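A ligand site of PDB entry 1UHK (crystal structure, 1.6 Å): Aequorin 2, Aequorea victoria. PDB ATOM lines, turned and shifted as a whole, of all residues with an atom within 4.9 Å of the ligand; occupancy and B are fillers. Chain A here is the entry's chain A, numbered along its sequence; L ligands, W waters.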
ATOM      1  N   HIS A  18     -25.850  29.133 -34.489  1.00  0.00           N
ATOM      2  CA  HIS A  18     -25.510  27.811 -33.956  1.00  0.00           C
ATOM      3  C   HIS A  18     -25.675  26.674 -34.970  1.00  0.00           C
ATOM      4  O   HIS A  18     -24.920  25.723 -34.896  1.00  0.00           O
ATOM      5  CB  HIS A  18     -26.178  27.552 -32.592  1.00  0.00           C
ATOM      6  CG  HIS A  18     -25.626  28.443 -31.523  1.00  0.00           C
ATOM      7  ND1 HIS A  18     -24.340  28.271 -31.008  1.00  0.00           N
ATOM      8  CD2 HIS A  18     -26.104  29.586 -30.966  1.00  0.00           C
ATOM      9  CE1 HIS A  18     -24.086  29.241 -30.144  1.00  0.00           C
ATOM     10  NE2 HIS A  18     -25.141  30.059 -30.112  1.00  0.00           N
ATOM     11  N   MET A  21     -22.521  26.636 -36.977  1.00  0.00           N
ATOM     12  CA  MET A  21     -21.437  25.984 -36.266  1.00  0.00           C
ATOM     13  C   MET A  21     -21.636  24.485 -36.191  1.00  0.00           C
ATOM     14  O   MET A  21     -20.634  23.739 -36.322  1.00  0.00           O
ATOM     15  CB  MET A  21     -21.289  26.564 -34.873  1.00  0.00           C
ATOM     16  CG  MET A  21     -20.772  28.020 -34.852  1.00  0.00           C
ATOM     17  SD  MET A  21     -19.256  28.273 -35.741  1.00  0.00           S
ATOM     18  CE  MET A  21     -18.087  27.173 -34.815  1.00  0.00           C
ATOM     19  N   PHE A  24     -20.545  23.192 -39.481  1.00  0.00           N
ATOM     20  CA  PHE A  24     -19.094  23.332 -39.554  1.00  0.00           C
ATOM     21  C   PHE A  24     -18.418  22.222 -38.742  1.00  0.00           C
ATOM     22  O   PHE A  24     -17.366  21.676 -39.148  1.00  0.00           O
ATOM     23  CB  PHE A  24     -18.664  24.730 -39.052  1.00  0.00           C
ATOM     24  CG  PHE A  24     -17.269  24.799 -38.580  1.00  0.00           C
ATOM     25  CD1 PHE A  24     -16.200  24.837 -39.469  1.00  0.00           C
ATOM     26  CD2 PHE A  24     -17.002  24.817 -37.223  1.00  0.00           C
ATOM     27  CE1 PHE A  24     -14.906  24.894 -38.990  1.00  0.00           C
ATOM     28  CE2 PHE A  24     -15.710  24.846 -36.762  1.00  0.00           C
ATOM     29  CZ  PHE A  24     -14.675  24.888 -37.660  1.00  0.00           C
ATOM     30  N   LEU A  25     -19.022  21.872 -37.610  1.00  0.00           N
ATOM     31  CA  LEU A  25     -18.480  20.796 -36.750  1.00  0.00           C
ATOM     32  C   LEU A  25     -18.757  19.413 -37.305  1.00  0.00           C
ATOM     33  O   LEU A  25     -17.984  18.505 -37.059  1.00  0.00           O
ATOM     34  CB  LEU A  25     -18.994  20.920 -35.325  1.00  0.00           C
ATOM     35  CG  LEU A  25     -18.405  22.147 -34.598  1.00  0.00           C
ATOM     36  CD1 LEU A  25     -19.101  22.327 -33.297  1.00  0.00           C
ATOM     37  CD2 LEU A  25     -16.870  22.059 -34.428  1.00  0.00           C
ATOM     38  N   MET A  38     -15.511  16.414 -30.619  1.00  0.00           N
ATOM     39  CA  MET A  38     -15.181  17.782 -30.199  1.00  0.00           C
ATOM     40  C   MET A  38     -13.869  17.852 -29.430  1.00  0.00           C
ATOM     41  O   MET A  38     -13.057  18.757 -29.685  1.00  0.00           O
ATOM     42  CB  MET A  38     -16.282  18.391 -29.334  1.00  0.00           C
ATOM     43  CG  MET A  38     -17.657  18.468 -29.969  1.00  0.00           C
ATOM     44  SD  MET A  38     -17.719  19.378 -31.460  1.00  0.00           S
ATOM     45  CE  MET A  38     -17.444  18.066 -32.698  1.00  0.00           C
ATOM     46  N   LYS A  41     -10.939  17.118 -31.921  1.00  0.00           N
ATOM     47  CA  LYS A  41     -10.634  18.312 -32.703  1.00  0.00           C
ATOM     48  C   LYS A  41      -9.832  19.334 -31.888  1.00  0.00           C
ATOM     49  O   LYS A  41      -8.840  19.857 -32.399  1.00  0.00           O
ATOM     50  CB  LYS A  41     -11.954  18.969 -33.182  1.00  0.00           C
ATOM     51  CG  LYS A  41     -11.740  20.230 -34.017  1.00  0.00           C
ATOM     52  CD  LYS A  41     -13.028  20.962 -34.411  1.00  0.00           C
ATOM     53  CE  LYS A  41     -12.783  22.268 -35.223  1.00  0.00           C
ATOM     54  NZ  LYS A  41     -12.404  22.056 -36.667  1.00  0.00           N
ATOM     55  N   ALA A  42     -10.270  19.584 -30.655  1.00  0.00           N
ATOM     56  CA  ALA A  42      -9.605  20.537 -29.786  1.00  0.00           C
ATOM     57  C   ALA A  42      -8.146  20.202 -29.551  1.00  0.00           C
ATOM     58  O   ALA A  42      -7.282  21.070 -29.601  1.00  0.00           O
ATOM     59  CB  ALA A  42     -10.331  20.634 -28.449  1.00  0.00           C
ATOM     60  N   ILE A  45      -5.891  20.375 -32.792  1.00  0.00           N
ATOM     61  CA  ILE A  45      -5.468  21.739 -33.105  1.00  0.00           C
ATOM     62  C   ILE A  45      -4.298  22.167 -32.203  1.00  0.00           C
ATOM     63  O   ILE A  45      -3.249  22.614 -32.716  1.00  0.00           O
ATOM     64  CB  ILE A  45      -6.619  22.735 -32.929  1.00  0.00           C
ATOM     65  CG1 ILE A  45      -7.703  22.557 -33.974  1.00  0.00           C
ATOM     66  CG2 ILE A  45      -6.113  24.176 -32.996  1.00  0.00           C
ATOM     67  CD1 ILE A  45      -9.055  23.038 -33.515  1.00  0.00           C
ATOM     68  N   VAL A  64     -12.712  22.342 -23.023  1.00  0.00           N
ATOM     69  CA  VAL A  64     -13.611  22.049 -24.154  1.00  0.00           C
ATOM     70  C   VAL A  64     -14.636  20.962 -23.788  1.00  0.00           C
ATOM     71  O   VAL A  64     -15.819  21.086 -24.120  1.00  0.00           O
ATOM     72  CB  VAL A  64     -12.798  21.676 -25.457  1.00  0.00           C
ATOM     73  CG1 VAL A  64     -13.697  21.100 -26.532  1.00  0.00           C
ATOM     74  CG2 VAL A  64     -12.006  22.890 -25.924  1.00  0.00           C
ATOM     75  N   PHE A  67     -17.229  22.605 -21.764  1.00  0.00           N
ATOM     76  CA  PHE A  67     -18.018  23.570 -22.561  1.00  0.00           C
ATOM     77  C   PHE A  67     -19.141  22.853 -23.326  1.00  0.00           C
ATOM     78  O   PHE A  67     -20.340  23.126 -23.112  1.00  0.00           O
ATOM     79  CB  PHE A  67     -17.098  24.344 -23.525  1.00  0.00           C
ATOM     80  CG  PHE A  67     -17.801  25.369 -24.359  1.00  0.00           C
ATOM     81  CD1 PHE A  67     -18.088  26.635 -23.852  1.00  0.00           C
ATOM     82  CD2 PHE A  67     -18.221  25.047 -25.634  1.00  0.00           C
ATOM     83  CE1 PHE A  67     -18.767  27.558 -24.635  1.00  0.00           C
ATOM     84  CE2 PHE A  67     -18.885  25.990 -26.414  1.00  0.00           C
ATOM     85  CZ  PHE A  67     -19.159  27.242 -25.894  1.00  0.00           C
ATOM     86  N   PHE A  68     -18.764  21.886 -24.163  1.00  0.00           N
ATOM     87  CA  PHE A  68     -19.760  21.101 -24.895  1.00  0.00           C
ATOM     88  C   PHE A  68     -20.598  20.197 -23.982  1.00  0.00           C
ATOM     89  O   PHE A  68     -21.770  19.926 -24.266  1.00  0.00           O
ATOM     90  CB  PHE A  68     -19.115  20.356 -26.063  1.00  0.00           C
ATOM     91  CG  PHE A  68     -18.631  21.277 -27.143  1.00  0.00           C
ATOM     92  CD1 PHE A  68     -17.284  21.570 -27.290  1.00  0.00           C
ATOM     93  CD2 PHE A  68     -19.549  21.890 -28.015  1.00  0.00           C
ATOM     94  CE1 PHE A  68     -16.836  22.456 -28.263  1.00  0.00           C
ATOM     95  CE2 PHE A  68     -19.107  22.782 -29.023  1.00  0.00           C
ATOM     96  CZ  PHE A  68     -17.776  23.055 -29.160  1.00  0.00           C
ATOM     97  N   TYR A  84     -28.997  19.262 -29.956  1.00  0.00           N
ATOM     98  CA  TYR A  84     -27.882  20.212 -29.887  1.00  0.00           C
ATOM     99  C   TYR A  84     -28.378  21.603 -29.544  1.00  0.00           C
ATOM    100  O   TYR A  84     -27.863  22.248 -28.637  1.00  0.00           O
ATOM    101  CB  TYR A  84     -27.123  20.243 -31.210  1.00  0.00           C
ATOM    102  CG  TYR A  84     -25.944  21.149 -31.223  1.00  0.00           C
ATOM    103  CD1 TYR A  84     -24.746  20.743 -30.655  1.00  0.00           C
ATOM    104  CD2 TYR A  84     -25.998  22.393 -31.802  1.00  0.00           C
ATOM    105  CE1 TYR A  84     -23.609  21.572 -30.675  1.00  0.00           C
ATOM    106  CE2 TYR A  84     -24.867  23.226 -31.843  1.00  0.00           C
ATOM    107  CZ  TYR A  84     -23.685  22.809 -31.263  1.00  0.00           C
ATOM    108  OH  TYR A  84     -22.554  23.601 -31.232  1.00  0.00           O
ATOM    109  N   TRP A  88     -27.931  23.869 -26.179  1.00  0.00           N
ATOM    110  CA  TRP A  88     -27.313  25.210 -26.263  1.00  0.00           C
ATOM    111  C   TRP A  88     -28.149  26.253 -25.525  1.00  0.00           C
ATOM    112  O   TRP A  88     -27.621  27.164 -24.885  1.00  0.00           O
ATOM    113  CB  TRP A  88     -27.032  25.621 -27.733  1.00  0.00           C
ATOM    114  CG  TRP A  88     -25.590  25.557 -28.052  1.00  0.00           C
ATOM    115  CD1 TRP A  88     -24.923  24.541 -28.615  1.00  0.00           C
ATOM    116  CD2 TRP A  88     -24.620  26.564 -27.752  1.00  0.00           C
ATOM    117  NE1 TRP A  88     -23.590  24.849 -28.719  1.00  0.00           N
ATOM    118  CE2 TRP A  88     -23.375  26.089 -28.195  1.00  0.00           C
ATOM    119  CE3 TRP A  88     -24.674  27.847 -27.165  1.00  0.00           C
ATOM    120  CZ2 TRP A  88     -22.208  26.842 -28.067  1.00  0.00           C
ATOM    121  CZ3 TRP A  88     -23.530  28.576 -27.064  1.00  0.00           C
ATOM    122  CH2 TRP A  88     -22.320  28.090 -27.546  1.00  0.00           C
ATOM    123  N   ILE A 107     -16.913  29.545 -21.044  1.00  0.00           N
ATOM    124  CA  ILE A 107     -16.263  30.166 -22.182  1.00  0.00           C
ATOM    125  C   ILE A 107     -14.970  30.881 -21.753  1.00  0.00           C
ATOM    126  O   ILE A 107     -13.952  30.767 -22.425  1.00  0.00           O
ATOM    127  CB  ILE A 107     -17.271  31.056 -23.017  1.00  0.00           C
ATOM    128  CG1 ILE A 107     -16.615  31.512 -24.338  1.00  0.00           C
ATOM    129  CG2 ILE A 107     -17.790  32.227 -22.236  1.00  0.00           C
ATOM    130  CD1 ILE A 107     -16.298  30.383 -25.281  1.00  0.00           C
ATOM    131  N   ARG A 108     -14.976  31.543 -20.599  1.00  0.00           N
ATOM    132  CA  ARG A 108     -13.753  32.158 -20.074  1.00  0.00           C
ATOM    133  C   ARG A 108     -12.712  31.112 -19.748  1.00  0.00           C
ATOM    134  O   ARG A 108     -11.545  31.309 -20.028  1.00  0.00           O
ATOM    135  CB  ARG A 108     -14.067  32.993 -18.817  1.00  0.00           C
ATOM    136  CG  ARG A 108     -12.855  33.634 -18.138  1.00  0.00           C
ATOM    137  CD  ARG A 108     -12.003  34.465 -19.040  1.00  0.00           C
ATOM    138  NE  ARG A 108     -10.822  35.054 -18.399  1.00  0.00           N
ATOM    139  CZ  ARG A 108     -10.722  36.319 -17.971  1.00  0.00           C
ATOM    140  NH1 ARG A 108     -11.752  37.147 -18.015  1.00  0.00           N
ATOM    141  NH2 ARG A 108      -9.575  36.736 -17.437  1.00  0.00           N
ATOM    142  N   TRP A 110     -12.263  28.246 -21.086  1.00  0.00           N
ATOM    143  CA  TRP A 110     -11.689  27.830 -22.372  1.00  0.00           C
ATOM    144  C   TRP A 110     -10.717  28.896 -22.902  1.00  0.00           C
ATOM    145  O   TRP A 110      -9.585  28.602 -23.266  1.00  0.00           O
ATOM    146  CB  TRP A 110     -12.836  27.536 -23.360  1.00  0.00           C
ATOM    147  CG  TRP A 110     -12.434  27.008 -24.680  1.00  0.00           C
ATOM    148  CD1 TRP A 110     -11.157  26.651 -25.110  1.00  0.00           C
ATOM    149  CD2 TRP A 110     -13.302  26.760 -25.789  1.00  0.00           C
ATOM    150  NE1 TRP A 110     -11.206  26.188 -26.401  1.00  0.00           N
ATOM    151  CE2 TRP A 110     -12.512  26.238 -26.843  1.00  0.00           C
ATOM    152  CE3 TRP A 110     -14.688  26.893 -26.001  1.00  0.00           C
ATOM    153  CZ2 TRP A 110     -13.045  25.877 -28.066  1.00  0.00           C
ATOM    154  CZ3 TRP A 110     -15.214  26.530 -27.216  1.00  0.00           C
ATOM    155  CH2 TRP A 110     -14.404  26.021 -28.232  1.00  0.00           C
ATOM    156  N   GLY A 111     -11.131  30.173 -22.908  1.00  0.00           N
ATOM    157  CA  GLY A 111     -10.287  31.260 -23.370  1.00  0.00           C
ATOM    158  C   GLY A 111      -8.948  31.302 -22.633  1.00  0.00           C
ATOM    159  O   GLY A 111      -7.912  31.483 -23.251  1.00  0.00           O
ATOM    160  N   LEU A 114      -6.823  28.332 -23.839  1.00  0.00           N
ATOM    161  CA  LEU A 114      -6.373  28.539 -25.209  1.00  0.00           C
ATOM    162  C   LEU A 114      -5.330  29.640 -25.285  1.00  0.00           C
ATOM    163  O   LEU A 114      -4.303  29.481 -25.935  1.00  0.00           O
ATOM    164  CB  LEU A 114      -7.562  28.802 -26.164  1.00  0.00           C
ATOM    165  CG  LEU A 114      -7.218  28.964 -27.639  1.00  0.00           C
ATOM    166  CD1 LEU A 114      -6.442  27.738 -28.214  1.00  0.00           C
ATOM    167  CD2 LEU A 114      -8.448  29.293 -28.471  1.00  0.00           C
ATOM    168  N   PHE A 115      -5.599  30.769 -24.633  1.00  0.00           N
ATOM    169  CA  PHE A 115      -4.663  31.884 -24.677  1.00  0.00           C
ATOM    170  C   PHE A 115      -3.297  31.556 -24.052  1.00  0.00           C
ATOM    171  O   PHE A 115      -2.289  32.139 -24.439  1.00  0.00           O
ATOM    172  CB  PHE A 115      -5.253  33.146 -24.043  1.00  0.00           C
ATOM    173  CG  PHE A 115      -6.094  33.956 -24.982  1.00  0.00           C
ATOM    174  CD1 PHE A 115      -6.819  33.356 -26.001  1.00  0.00           C
ATOM    175  CD2 PHE A 115      -6.142  35.325 -24.875  1.00  0.00           C
ATOM    176  CE1 PHE A 115      -7.596  34.119 -26.871  1.00  0.00           C
ATOM    177  CE2 PHE A 115      -6.939  36.081 -25.755  1.00  0.00           C
ATOM    178  CZ  PHE A 115      -7.631  35.482 -26.737  1.00  0.00           C
ATOM    179  N   TRP A 131      -4.221  35.265 -33.678  1.00  0.00           N
ATOM    180  CA  TRP A 131      -5.643  34.992 -33.939  1.00  0.00           C
ATOM    181  C   TRP A 131      -5.837  34.309 -35.301  1.00  0.00           C
ATOM    182  O   TRP A 131      -6.665  33.374 -35.424  1.00  0.00           O
ATOM    183  CB  TRP A 131      -6.446  36.322 -33.880  1.00  0.00           C
ATOM    184  CG  TRP A 131      -7.953  36.224 -34.105  1.00  0.00           C
ATOM    185  CD1 TRP A 131      -8.677  36.901 -35.043  1.00  0.00           C
ATOM    186  CD2 TRP A 131      -8.881  35.409 -33.391  1.00  0.00           C
ATOM    187  NE1 TRP A 131     -10.006  36.555 -34.952  1.00  0.00           N
ATOM    188  CE2 TRP A 131     -10.172  35.658 -33.938  1.00  0.00           C
ATOM    189  CE3 TRP A 131      -8.773  34.499 -32.314  1.00  0.00           C
ATOM    190  CZ2 TRP A 131     -11.329  35.040 -33.450  1.00  0.00           C
ATOM    191  CZ3 TRP A 131      -9.945  33.865 -31.843  1.00  0.00           C
ATOM    192  CH2 TRP A 131     -11.198  34.143 -32.405  1.00  0.00           C
ATOM    193  N   TYR A 134      -4.717  30.557 -34.861  1.00  0.00           N
ATOM    194  CA  TYR A 134      -5.707  29.743 -34.187  1.00  0.00           C
ATOM    195  C   TYR A 134      -6.915  29.512 -35.089  1.00  0.00           C
ATOM    196  O   TYR A 134      -7.317  28.374 -35.320  1.00  0.00           O
ATOM    197  CB  TYR A 134      -6.153  30.341 -32.837  1.00  0.00           C
ATOM    198  CG  TYR A 134      -7.359  29.559 -32.369  1.00  0.00           C
ATOM    199  CD1 TYR A 134      -7.237  28.206 -31.975  1.00  0.00           C
ATOM    200  CD2 TYR A 134      -8.636  30.081 -32.466  1.00  0.00           C
ATOM    201  CE1 TYR A 134      -8.352  27.438 -31.644  1.00  0.00           C
ATOM    202  CE2 TYR A 134      -9.765  29.313 -32.135  1.00  0.00           C
ATOM    203  CZ  TYR A 134      -9.612  27.995 -31.720  1.00  0.00           C
ATOM    204  OH  TYR A 134     -10.714  27.208 -31.405  1.00  0.00           O
ATOM    205  N   ALA A 138      -8.259  25.914 -36.664  1.00  0.00           N
ATOM    206  CA  ALA A 138      -9.568  25.369 -36.295  1.00  0.00           C
ATOM    207  C   ALA A 138     -10.469  25.325 -37.518  1.00  0.00           C
ATOM    208  O   ALA A 138     -11.320  24.441 -37.634  1.00  0.00           O
ATOM    209  CB  ALA A 138     -10.202  26.199 -35.214  1.00  0.00           C
ATOM    210  N   ILE A 140     -12.537  27.867 -38.200  1.00  0.00           N
ATOM    211  CA  ILE A 140     -13.691  28.726 -37.930  1.00  0.00           C
ATOM    212  C   ILE A 140     -13.680  30.025 -38.763  1.00  0.00           C
ATOM    213  O   ILE A 140     -14.755  30.524 -39.145  1.00  0.00           O
ATOM    214  CB  ILE A 140     -13.886  28.952 -36.416  1.00  0.00           C
ATOM    215  CG1 ILE A 140     -15.248  29.577 -36.093  1.00  0.00           C
ATOM    216  CG2 ILE A 140     -12.756  29.753 -35.803  1.00  0.00           C
ATOM    217  CD1 ILE A 140     -15.581  29.616 -34.608  1.00  0.00           C
ATOM    218  N   VAL A 164      -8.121  38.512 -23.255  1.00  0.00           N
ATOM    219  CA  VAL A 164      -9.075  37.463 -22.973  1.00  0.00           C
ATOM    220  C   VAL A 164     -10.354  37.969 -22.327  1.00  0.00           C
ATOM    221  O   VAL A 164     -11.423  37.435 -22.602  1.00  0.00           O
ATOM    222  CB  VAL A 164      -8.424  36.344 -22.099  1.00  0.00           C
ATOM    223  CG1 VAL A 164      -8.117  36.824 -20.669  1.00  0.00           C
ATOM    224  CG2 VAL A 164      -9.316  35.081 -22.103  1.00  0.00           C
ATOM    225  N   MET A 167     -12.441  39.536 -25.194  1.00  0.00           N
ATOM    226  CA  MET A 167     -12.970  38.502 -26.082  1.00  0.00           C
ATOM    227  C   MET A 167     -14.034  37.674 -25.399  1.00  0.00           C
ATOM    228  O   MET A 167     -14.981  37.219 -26.057  1.00  0.00           O
ATOM    229  CB  MET A 167     -11.863  37.618 -26.688  1.00  0.00           C
ATOM    230  CG  MET A 167     -12.324  36.744 -27.849  1.00  0.00           C
ATOM    231  SD  MET A 167     -13.263  37.646 -29.130  1.00  0.00           S
ATOM    232  CE  MET A 167     -13.007  36.643 -30.580  1.00  0.00           C
ATOM    233  N   THR A 168     -13.937  37.518 -24.078  1.00  0.00           N
ATOM    234  CA  THR A 168     -14.964  36.799 -23.334  1.00  0.00           C
ATOM    235  C   THR A 168     -16.274  37.584 -23.406  1.00  0.00           C
ATOM    236  O   THR A 168     -17.318  37.015 -23.671  1.00  0.00           O
ATOM    237  CB  THR A 168     -14.567  36.566 -21.879  1.00  0.00           C
ATOM    238  OG1 THR A 168     -13.444  35.668 -21.827  1.00  0.00           O
ATOM    239  CG2 THR A 168     -15.662  35.890 -21.117  1.00  0.00           C
ATOM    240  N   HIS A 171     -17.707  37.206 -26.864  1.00  0.00           N
ATOM    241  CA  HIS A 171     -18.287  35.876 -27.006  1.00  0.00           C
ATOM    242  C   HIS A 171     -19.627  35.734 -26.333  1.00  0.00           C
ATOM    243  O   HIS A 171     -20.493  35.058 -26.855  1.00  0.00           O
ATOM    244  CB  HIS A 171     -17.311  34.802 -26.530  1.00  0.00           C
ATOM    245  CG  HIS A 171     -16.309  34.424 -27.580  1.00  0.00           C
ATOM    246  ND1 HIS A 171     -15.147  33.748 -27.277  1.00  0.00           N
ATOM    247  CD2 HIS A 171     -16.279  34.641 -28.906  1.00  0.00           C
ATOM    248  CE1 HIS A 171     -14.461  33.547 -28.381  1.00  0.00           C
ATOM    249  NE2 HIS A 171     -15.117  34.088 -29.387  1.00  0.00           N
ATOM    250  N   TRP A 175     -22.247  34.557 -28.975  1.00  0.00           N
ATOM    251  CA  TRP A 175     -22.768  33.202 -28.859  1.00  0.00           C
ATOM    252  C   TRP A 175     -24.035  33.093 -27.984  1.00  0.00           C
ATOM    253  O   TRP A 175     -24.841  32.216 -28.168  1.00  0.00           O
ATOM    254  CB  TRP A 175     -21.712  32.244 -28.318  1.00  0.00           C
ATOM    255  CG  TRP A 175     -20.422  32.096 -29.124  1.00  0.00           C
ATOM    256  CD1 TRP A 175     -19.155  32.246 -28.639  1.00  0.00           C
ATOM    257  CD2 TRP A 175     -20.279  31.744 -30.509  1.00  0.00           C
ATOM    258  NE1 TRP A 175     -18.234  32.018 -29.634  1.00  0.00           N
ATOM    259  CE2 TRP A 175     -18.900  31.700 -30.793  1.00  0.00           C
ATOM    260  CE3 TRP A 175     -21.185  31.424 -31.531  1.00  0.00           C
ATOM    261  CZ2 TRP A 175     -18.404  31.378 -32.055  1.00  0.00           C
ATOM    262  CZ3 TRP A 175     -20.694  31.122 -32.783  1.00  0.00           C
ATOM    263  CH2 TRP A 175     -19.300  31.104 -33.047  1.00  0.00           C
ATOM    264  N   TYR A 186     -16.638  37.409 -36.160  1.00  0.00           N
ATOM    265  CA  TYR A 186     -15.886  36.501 -36.996  1.00  0.00           C
ATOM    266  C   TYR A 186     -15.945  36.920 -38.468  1.00  0.00           C
ATOM    267  O   TYR A 186     -15.736  36.103 -39.391  1.00  0.00           O
ATOM    268  CB  TYR A 186     -16.378  35.036 -36.781  1.00  0.00           C
ATOM    269  CG  TYR A 186     -15.967  34.446 -35.452  1.00  0.00           C
ATOM    270  CD1 TYR A 186     -16.676  34.731 -34.293  1.00  0.00           C
ATOM    271  CD2 TYR A 186     -14.882  33.617 -35.363  1.00  0.00           C
ATOM    272  CE1 TYR A 186     -16.267  34.210 -33.083  1.00  0.00           C
ATOM    273  CE2 TYR A 186     -14.478  33.102 -34.188  1.00  0.00           C
ATOM    274  CZ  TYR A 186     -15.163  33.400 -33.061  1.00  0.00           C
ATOM    275  OH  TYR A 186     -14.712  32.863 -31.894  1.00  0.00           O
HETATM  276  O1  LIG L   1     -15.089  30.735 -29.145  1.00  0.00           O
HETATM  277  C1  LIG L   1     -14.575  29.861 -29.810  1.00  0.00           C
HETATM  278  N1  LIG L   1     -15.291  28.859 -30.410  1.00  0.00           N
HETATM  279  C2  LIG L   1     -16.626  28.641 -30.422  1.00  0.00           C
HETATM  280  C3  LIG L   1     -14.452  28.054 -31.054  1.00  0.00           C
HETATM  281  C4  LIG L   1     -14.971  26.892 -31.775  1.00  0.00           C
HETATM  282  N2  LIG L   1     -16.282  26.710 -31.773  1.00  0.00           N
HETATM  283  C5  LIG L   1     -17.121  27.522 -31.114  1.00  0.00           C
HETATM  284  C6  LIG L   1     -18.574  27.217 -31.217  1.00  0.00           C
HETATM  285  C7  LIG L   1     -18.995  26.067 -31.874  1.00  0.00           C
HETATM  286  C8  LIG L   1     -20.336  25.733 -31.990  1.00  0.00           C
HETATM  287  C9  LIG L   1     -21.312  26.556 -31.451  1.00  0.00           C
HETATM  288  C10 LIG L   1     -20.897  27.700 -30.817  1.00  0.00           C
HETATM  289  C11 LIG L   1     -19.549  28.039 -30.678  1.00  0.00           C
HETATM  290  O2  LIG L   1     -22.631  26.224 -31.587  1.00  0.00           O
HETATM  291  C12 LIG L   1     -14.081  25.972 -32.548  1.00  0.00           C
HETATM  292  C13 LIG L   1     -13.837  24.652 -31.913  1.00  0.00           C
HETATM  293  C14 LIG L   1     -12.546  24.328 -31.535  1.00  0.00           C
HETATM  294  C15 LIG L   1     -12.285  23.106 -30.949  1.00  0.00           C
HETATM  295  C16 LIG L   1     -13.321  22.224 -30.717  1.00  0.00           C
HETATM  296  C17 LIG L   1     -14.604  22.556 -31.086  1.00  0.00           C
HETATM  297  C18 LIG L   1     -14.880  23.772 -31.689  1.00  0.00           C
HETATM  298  N3  LIG L   1     -13.185  28.441 -30.912  1.00  0.00           N
HETATM  299  C19 LIG L   1     -13.104  29.658 -30.106  1.00  0.00           C
HETATM  300  O3  LIG L   1     -12.735  30.754 -30.943  1.00  0.00           O
HETATM  301  O4  LIG L   1     -13.346  30.810 -32.063  1.00  0.00           O
HETATM  302  C20 LIG L   1     -12.125  29.436 -28.977  1.00  0.00           C
HETATM  303  C21 LIG L   1     -11.932  30.714 -28.162  1.00  0.00           C
HETATM  304  C22 LIG L   1     -12.593  30.846 -26.960  1.00  0.00           C
HETATM  305  C23 LIG L   1     -12.416  32.009 -26.185  1.00  0.00           C
HETATM  306  C24 LIG L   1     -13.093  32.195 -24.997  1.00  0.00           C
HETATM  307  C25 LIG L   1     -11.503  33.049 -26.708  1.00  0.00           C
HETATM  308  C26 LIG L   1     -10.882  32.872 -27.926  1.00  0.00           C
HETATM  309  C27 LIG L   1     -11.077  31.690 -28.633  1.00  0.00           C
HETATM  310  C28 LIG L   1     -11.325  34.216 -25.961  1.00  0.00           C
HETATM  311  C29 LIG L   1     -12.006  34.369 -24.749  1.00  0.00           C
HETATM  312  C30 LIG L   1     -12.872  33.361 -24.262  1.00  0.00           C
HETATM  313  O   HOH W   1      -9.877  25.313 -29.508  1.00  0.00           O
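Merely in contact with the ligand: Ile 107 (3.1 Å), Met 21 (3.1 Å), Met 167 (3.3 Å), Gly 111 (3.4 Å), Thr 168 (3.4 Å), Trp 110 (3.5 Å), Leu 114 (3.6 Å), Ile 140 (3.6 Å), Phe 68 (3.6 Å), Met 38 (3.6 Å), Phe 115 (3.7 Å), Val 164 (3.8 Å), Leu 25 (3.8 Å), Ala 42 (3.9 Å), Lys 41 (3.9 Å) and Trp 131 (3.98 Å).
The side-chain amino group (NZ) of Lys 41 sits at hydrogen-bond distance from the backbone carbonyl oxygen (O) of Ala 138, at 2.8 Å.
The indole nitrogen (NE1) of Trp 88 lies within hydrogen-bond range of the side-chain hydroxyl (OH) of Tyr 84.
OH of Tyr 186 lies within hydrogen-bond range of NE2 of His 171 (2.8 Å).
O of Trp 175 sits at hydrogen-bond distance from NE2 of His 18.
The side-chain hydroxyl (OG1) of Thr 168 sits at hydrogen-bond distance from the backbone carbonyl oxygen (O) of Val 164 (2.8 Å).
An oxygen (O2) of the ligand sits at hydrogen-bond distance from a ring nitrogen (ND1) of His 18, at 2.7 Å.
NE1 of Trp 175 sits at hydrogen-bond distance from O1 of the ligand (3.4 Å).
OH of Tyr 134 sits at hydrogen-bond distance from N3 of the ligand (2.8 Å).
The indole nitrogen of Trp 88 is in hydrogen-bond range of an oxygen (O2) of the ligand (3.3 Å).
A ring nitrogen (NE2) of His 171 lies close to an oxygen (O1) of the ligand.
The side-chain hydroxyl (OH) of Tyr 186 lies within hydrogen-bond range of an oxygen (O4) of the ligand (2.5 Å).
OH of Tyr 84 sits at hydrogen-bond distance from O2 of the ligand (2.6 Å).
Water W1 lies within hydrogen-bond range of OH of Tyr 134 (2.8 Å) and NE1 of Trp 110 (3.5 Å).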
